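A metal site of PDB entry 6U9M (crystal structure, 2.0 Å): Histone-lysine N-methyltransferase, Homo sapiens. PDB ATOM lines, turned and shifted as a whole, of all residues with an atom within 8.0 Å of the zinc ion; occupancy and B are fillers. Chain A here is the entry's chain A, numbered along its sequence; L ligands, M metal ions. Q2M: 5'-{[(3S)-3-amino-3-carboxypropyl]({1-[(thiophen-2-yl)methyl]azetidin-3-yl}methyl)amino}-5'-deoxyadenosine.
The backbone carbonyl oxygen (O) of His 96 sits at hydrogen-bond distance from a nitrogen (N) of the ligand. The backbone NH (N) of His 96 sits at hydrogen-bond distance from a nitrogen (N3) of the ligand. The side-chain sulfur of Cys 146 sits close to a nitrogen (N) of the ligand, 3.5 Å away. N of Asn 147 is in hydrogen-bond range of N1 of the ligand (2.9 Å).
The side-chain sulfur (SG) of Cys 98 sits close to a ring nitrogen (NE2) of His 96, at 3.6 Å. N of Cys 146 is in hydrogen-bond range of O of Lys 155. N of Arg 154 sits close to SG of Cys 98 (3.2 Å). The backbone NH (N) of Lys 155 lies close to the side-chain sulfur (SG) of Cys 153. The side-chain sulfur (SG) of Cys 148 sits close to the backbone NH (N) of Ala 150.
Of the 19 residues printed, 4 come within 4 Å of the zinc ion.
The zinc ion is bound by SG of Cys 98, at 2.2 Å. SG of Cys 148 is bound to the zinc ion (2.3 Å). SG of Cys 146 is bound to the zinc ion (2.4 Å). SG of Cys 153 is bound to the zinc ion, at 2.5 Å. The zinc ion has four donor atoms within binding distance.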
ATOM      1  N   ILE A  27     -20.618  14.181 -28.638  1.00  0.00           N
ATOM      2  CA  ILE A  27     -19.259  13.758 -28.269  1.00  0.00           C
ATOM      3  C   ILE A  27     -18.988  12.456 -29.018  1.00  0.00           C
ATOM      4  O   ILE A  27     -18.038  12.397 -29.797  1.00  0.00           O
ATOM      5  CB  ILE A  27     -19.060  13.647 -26.720  1.00  0.00           C
ATOM      6  CG1 ILE A  27     -19.155  15.038 -26.043  1.00  0.00           C
ATOM      7  CG2 ILE A  27     -17.718  13.008 -26.395  1.00  0.00           C
ATOM      8  CD1 ILE A  27     -19.436  14.977 -24.448  1.00  0.00           C
ATOM      9  N   HIS A  96     -16.417  10.362 -22.148  1.00  0.00           N
ATOM     10  CA  HIS A  96     -15.280  11.072 -21.521  1.00  0.00           C
ATOM     11  C   HIS A  96     -15.357  12.583 -21.790  1.00  0.00           C
ATOM     12  O   HIS A  96     -15.812  12.981 -22.862  1.00  0.00           O
ATOM     13  CB  HIS A  96     -13.941  10.563 -22.103  1.00  0.00           C
ATOM     14  CG  HIS A  96     -12.753  11.400 -21.732  1.00  0.00           C
ATOM     15  ND1 HIS A  96     -12.140  11.259 -20.503  1.00  0.00           N
ATOM     16  CD2 HIS A  96     -12.163  12.415 -22.397  1.00  0.00           C
ATOM     17  CE1 HIS A  96     -11.172  12.154 -20.477  1.00  0.00           C
ATOM     18  NE2 HIS A  96     -11.148  12.882 -21.590  1.00  0.00           N
ATOM     19  N   SER A  97     -14.835  13.412 -20.854  1.00  0.00           N
ATOM     20  CA  SER A  97     -14.628  14.875 -21.013  1.00  0.00           C
ATOM     21  C   SER A  97     -13.456  15.325 -20.195  1.00  0.00           C
ATOM     22  O   SER A  97     -13.289  14.879 -19.064  1.00  0.00           O
ATOM     23  CB  SER A  97     -15.856  15.698 -20.653  1.00  0.00           C
ATOM     24  OG  SER A  97     -15.619  17.088 -20.846  1.00  0.00           O
ATOM     25  N   CYS A  98     -12.663  16.276 -20.743  1.00  0.00           N
ATOM     26  CA  CYS A  98     -11.482  16.870 -20.119  1.00  0.00           C
ATOM     27  C   CYS A  98     -11.874  17.911 -19.087  1.00  0.00           C
ATOM     28  O   CYS A  98     -11.041  18.350 -18.276  1.00  0.00           O
ATOM     29  CB  CYS A  98     -10.541  17.427 -21.184  1.00  0.00           C
ATOM     30  SG  CYS A  98     -10.088  16.213 -22.439  1.00  0.00           S
ATOM     31  N   GLU A  99     -13.146  18.300 -19.122  1.00  0.00           N
ATOM     32  CA  GLU A  99     -13.742  19.151 -18.100  1.00  0.00           C
ATOM     33  C   GLU A  99     -15.050  18.485 -17.716  1.00  0.00           C
ATOM     34  O   GLU A  99     -16.138  18.902 -18.141  1.00  0.00           O
ATOM     35  CB  GLU A  99     -13.890  20.603 -18.505  1.00  0.00           C
ATOM     36  CG  GLU A  99     -14.097  21.433 -17.260  1.00  0.00           C
ATOM     37  CD  GLU A  99     -13.992  22.920 -17.453  1.00  0.00           C
ATOM     38  OE1 GLU A  99     -14.634  23.655 -16.675  1.00  0.00           O
ATOM     39  OE2 GLU A  99     -13.265  23.354 -18.381  1.00  0.00           O
ATOM     40  N   ASP A 132     -13.753  11.908 -16.345  1.00  0.00           N
ATOM     41  CA  ASP A 132     -12.457  11.798 -16.978  1.00  0.00           C
ATOM     42  C   ASP A 132     -12.055  10.309 -17.009  1.00  0.00           C
ATOM     43  O   ASP A 132     -11.924   9.698 -15.944  1.00  0.00           O
ATOM     44  CB  ASP A 132     -11.415  12.613 -16.182  1.00  0.00           C
ATOM     45  CG  ASP A 132     -10.164  12.944 -16.966  1.00  0.00           C
ATOM     46  OD1 ASP A 132      -9.375  12.010 -17.240  1.00  0.00           O
ATOM     47  OD2 ASP A 132      -9.984  14.133 -17.324  1.00  0.00           O
ATOM     48  N   PRO A 145      -8.460  10.159 -30.330  1.00  0.00           N
ATOM     49  CA  PRO A 145      -8.818  11.596 -30.313  1.00  0.00           C
ATOM     50  C   PRO A 145     -10.059  11.954 -29.493  1.00  0.00           C
ATOM     51  O   PRO A 145     -11.085  11.296 -29.607  1.00  0.00           O
ATOM     52  CB  PRO A 145      -8.977  11.954 -31.798  1.00  0.00           C
ATOM     53  CG  PRO A 145      -9.232  10.673 -32.484  1.00  0.00           C
ATOM     54  CD  PRO A 145      -8.545   9.594 -31.693  1.00  0.00           C
ATOM     55  N   CYS A 146      -9.960  13.015 -28.671  1.00  0.00           N
ATOM     56  CA  CYS A 146     -11.052  13.468 -27.808  1.00  0.00           C
ATOM     57  C   CYS A 146     -11.956  14.506 -28.460  1.00  0.00           C
ATOM     58  O   CYS A 146     -11.479  15.517 -29.008  1.00  0.00           O
ATOM     59  CB  CYS A 146     -10.527  13.958 -26.464  1.00  0.00           C
ATOM     60  SG  CYS A 146     -11.832  14.350 -25.287  1.00  0.00           S
ATOM     61  N   ASN A 147     -13.270  14.285 -28.327  1.00  0.00           N
ATOM     62  CA  ASN A 147     -14.321  15.124 -28.894  1.00  0.00           C
ATOM     63  C   ASN A 147     -15.191  15.854 -27.836  1.00  0.00           C
ATOM     64  O   ASN A 147     -16.275  16.325 -28.164  1.00  0.00           O
ATOM     65  CB  ASN A 147     -15.182  14.304 -29.851  1.00  0.00           C
ATOM     66  CG  ASN A 147     -15.941  15.127 -30.852  1.00  0.00           C
ATOM     67  OD1 ASN A 147     -15.386  15.955 -31.585  1.00  0.00           O
ATOM     68  ND2 ASN A 147     -17.256  14.911 -30.907  1.00  0.00           N
ATOM     69  N   CYS A 148     -14.696  15.992 -26.585  1.00  0.00           N
ATOM     70  CA  CYS A 148     -15.464  16.688 -25.543  1.00  0.00           C
ATOM     71  C   CYS A 148     -15.735  18.161 -25.895  1.00  0.00           C
ATOM     72  O   CYS A 148     -16.734  18.725 -25.436  1.00  0.00           O
ATOM     73  CB  CYS A 148     -14.799  16.552 -24.174  1.00  0.00           C
ATOM     74  SG  CYS A 148     -13.339  17.598 -23.935  1.00  0.00           S
ATOM     75  N   GLY A 149     -14.815  18.756 -26.662  1.00  0.00           N
ATOM     76  CA  GLY A 149     -14.873  20.126 -27.140  1.00  0.00           C
ATOM     77  C   GLY A 149     -14.492  21.194 -26.136  1.00  0.00           C
ATOM     78  O   GLY A 149     -14.606  22.382 -26.455  1.00  0.00           O
ATOM     79  N   ALA A 150     -14.041  20.814 -24.914  1.00  0.00           N
ATOM     80  CA  ALA A 150     -13.665  21.768 -23.843  1.00  0.00           C
ATOM     81  C   ALA A 150     -12.504  22.706 -24.262  1.00  0.00           C
ATOM     82  O   ALA A 150     -11.686  22.333 -25.100  1.00  0.00           O
ATOM     83  CB  ALA A 150     -13.315  21.027 -22.561  1.00  0.00           C
ATOM     84  N   LYS A 151     -12.439  23.910 -23.675  1.00  0.00           N
ATOM     85  CA  LYS A 151     -11.348  24.834 -24.005  1.00  0.00           C
ATOM     86  C   LYS A 151      -9.996  24.185 -23.667  1.00  0.00           C
ATOM     87  O   LYS A 151      -9.066  24.197 -24.481  1.00  0.00           O
ATOM     88  CB  LYS A 151     -11.519  26.156 -23.217  1.00  0.00           C
ATOM     89  CG  LYS A 151     -10.450  27.218 -23.529  1.00  0.00           C
ATOM     90  N   LYS A 152      -9.919  23.571 -22.473  1.00  0.00           N
ATOM     91  CA  LYS A 152      -8.737  22.926 -21.909  1.00  0.00           C
ATOM     92  C   LYS A 152      -8.664  21.444 -22.237  1.00  0.00           C
ATOM     93  O   LYS A 152      -8.164  20.658 -21.432  1.00  0.00           O
ATOM     94  CB  LYS A 152      -8.693  23.197 -20.379  1.00  0.00           C
ATOM     95  CG  LYS A 152      -8.782  24.667 -19.973  1.00  0.00           C
ATOM     96  CD  LYS A 152      -7.445  25.394 -20.039  1.00  0.00           C
ATOM     97  CE  LYS A 152      -7.590  26.838 -19.594  1.00  0.00           C
ATOM     98  NZ  LYS A 152      -6.288  27.438 -19.211  1.00  0.00           N
ATOM     99  N   CYS A 153      -9.159  21.052 -23.428  1.00  0.00           N
ATOM    100  CA  CYS A 153      -9.172  19.667 -23.896  1.00  0.00           C
ATOM    101  C   CYS A 153      -7.750  19.093 -24.015  1.00  0.00           C
ATOM    102  O   CYS A 153      -6.883  19.753 -24.559  1.00  0.00           O
ATOM    103  CB  CYS A 153      -9.942  19.545 -25.199  1.00  0.00           C
ATOM    104  SG  CYS A 153     -10.061  17.852 -25.844  1.00  0.00           S
ATOM    105  N   ARG A 154      -7.536  17.865 -23.495  1.00  0.00           N
ATOM    106  CA  ARG A 154      -6.271  17.122 -23.558  1.00  0.00           C
ATOM    107  C   ARG A 154      -6.030  16.561 -24.983  1.00  0.00           C
ATOM    108  O   ARG A 154      -4.936  16.067 -25.271  1.00  0.00           O
ATOM    109  CB  ARG A 154      -6.253  15.987 -22.516  1.00  0.00           C
ATOM    110  N   LYS A 155      -7.075  16.619 -25.845  1.00  0.00           N
ATOM    111  CA  LYS A 155      -7.132  16.240 -27.268  1.00  0.00           C
ATOM    112  C   LYS A 155      -7.038  14.720 -27.537  1.00  0.00           C
ATOM    113  O   LYS A 155      -7.278  14.295 -28.673  1.00  0.00           O
ATOM    114  CB  LYS A 155      -6.098  17.031 -28.097  1.00  0.00           C
ATOM    115  CG  LYS A 155      -6.260  18.563 -27.972  1.00  0.00           C
ATOM    116  CD  LYS A 155      -7.553  19.084 -28.615  1.00  0.00           C
ATOM    117  CE  LYS A 155      -7.658  20.592 -28.567  1.00  0.00           C
ATOM    118  NZ  LYS A 155      -8.801  21.083 -29.397  1.00  0.00           N
ATOM    119  N   PHE A 156      -6.748  13.914 -26.479  1.00  0.00           N
ATOM    120  CA  PHE A 156      -6.675  12.442 -26.533  1.00  0.00           C
ATOM    121  C   PHE A 156      -7.216  11.809 -25.235  1.00  0.00           C
ATOM    122  O   PHE A 156      -7.094  12.425 -24.173  1.00  0.00           O
ATOM    123  CB  PHE A 156      -5.252  11.944 -26.847  1.00  0.00           C
ATOM    124  CG  PHE A 156      -4.731  12.375 -28.193  1.00  0.00           C
ATOM    125  CD1 PHE A 156      -5.138  11.735 -29.358  1.00  0.00           C
ATOM    126  CD2 PHE A 156      -3.878  13.479 -28.303  1.00  0.00           C
ATOM    127  CE1 PHE A 156      -4.681  12.170 -30.605  1.00  0.00           C
ATOM    128  CE2 PHE A 156      -3.434  13.919 -29.551  1.00  0.00           C
ATOM    129  CZ  PHE A 156      -3.836  13.254 -30.694  1.00  0.00           C
ATOM    130  N   LEU A 157      -7.826  10.609 -25.330  1.00  0.00           N
ATOM    131  CA  LEU A 157      -8.377   9.924 -24.152  1.00  0.00           C
ATOM    132  C   LEU A 157      -7.258   9.326 -23.280  1.00  0.00           C
ATOM    133  O   LEU A 157      -7.366   9.332 -22.052  1.00  0.00           O
ATOM    134  CB  LEU A 157      -9.384   8.823 -24.524  1.00  0.00           C
ATOM    135  CG  LEU A 157     -10.548   9.155 -25.485  1.00  0.00           C
ATOM    136  CD1 LEU A 157     -11.377   7.922 -25.728  1.00  0.00           C
ATOM    137  CD2 LEU A 157     -11.445  10.243 -24.951  1.00  0.00           C
HETATM  138  C1  Q2M L   1     -14.166  10.642 -28.507  1.00  0.00           C
HETATM  139  C2  Q2M L   1     -15.222   9.149 -27.138  1.00  0.00           C
HETATM  140  C3  Q2M L   1     -15.282  10.115 -26.085  1.00  0.00           C
HETATM  141  C4  Q2M L   1     -16.271   8.350 -25.313  1.00  0.00           C
HETATM  142  C5  Q2M L   1     -15.906   6.694 -27.260  1.00  0.00           C
HETATM  143  C6  Q2M L   1     -14.508   5.990 -27.206  1.00  0.00           C
HETATM  144  C7  Q2M L   1     -14.650   5.215 -25.887  1.00  0.00           C
HETATM  145  C8  Q2M L   1     -16.113   4.765 -26.016  1.00  0.00           C
HETATM  146  O1  Q2M L   1     -13.780   4.129 -25.778  1.00  0.00           O
HETATM  147  N1  Q2M L   1     -14.132  11.665 -27.574  1.00  0.00           N
HETATM  148  N2  Q2M L   1     -14.663   9.378 -28.385  1.00  0.00           N
HETATM  149  N   Q2M L   1     -14.649  12.351 -25.393  1.00  0.00           N
HETATM  150  C   Q2M L   1     -14.689  11.397 -26.344  1.00  0.00           C
HETATM  151  O   Q2M L   1     -14.471   5.170 -28.326  1.00  0.00           O
HETATM  152  O3  Q2M L   1     -21.766   3.187 -26.643  1.00  0.00           O
HETATM  153  C22 Q2M L   1     -21.600   4.382 -26.867  1.00  0.00           C
HETATM  154  O2  Q2M L   1     -22.406   4.997 -27.751  1.00  0.00           O
HETATM  155  C21 Q2M L   1     -20.507   5.294 -26.246  1.00  0.00           C
HETATM  156  N7  Q2M L   1     -20.722   6.725 -26.525  1.00  0.00           N
HETATM  157  C20 Q2M L   1     -20.529   5.059 -24.690  1.00  0.00           C
HETATM  158  C19 Q2M L   1     -19.098   5.058 -24.075  1.00  0.00           C
HETATM  159  N5  Q2M L   1     -18.172   4.069 -24.796  1.00  0.00           N
HETATM  160  C10 Q2M L   1     -18.485   2.606 -24.597  1.00  0.00           C
HETATM  161  C11 Q2M L   1     -17.896   1.788 -25.794  1.00  0.00           C
HETATM  162  C18 Q2M L   1     -18.482   0.388 -26.147  1.00  0.00           C
HETATM  163  N6  Q2M L   1     -18.556   0.802 -27.612  1.00  0.00           N
HETATM  164  C13 Q2M L   1     -19.801   0.439 -28.351  1.00  0.00           C
HETATM  165  C14 Q2M L   1     -19.808   1.125 -29.679  1.00  0.00           C
HETATM  166  S   Q2M L   1     -18.370   1.266 -30.635  1.00  0.00           S
HETATM  167  C17 Q2M L   1     -19.195   2.141 -31.856  1.00  0.00           C
HETATM  168  C16 Q2M L   1     -20.497   2.323 -31.563  1.00  0.00           C
HETATM  169  C15 Q2M L   1     -20.867   1.726 -30.299  1.00  0.00           C
HETATM  170  C12 Q2M L   1     -18.409   2.239 -27.210  1.00  0.00           C
HETATM  171  C9  Q2M L   1     -16.706   4.424 -24.621  1.00  0.00           C
HETATM  172  O4  Q2M L   1     -16.823   5.858 -26.617  1.00  0.00           O
HETATM  173  N4  Q2M L   1     -15.835   8.015 -26.635  1.00  0.00           N
HETATM  174  N3  Q2M L   1     -15.949   9.587 -24.964  1.00  0.00           N
HETATM  175 ZN    ZN M   1     -11.380  16.492 -24.242  1.00  0.00          ZN
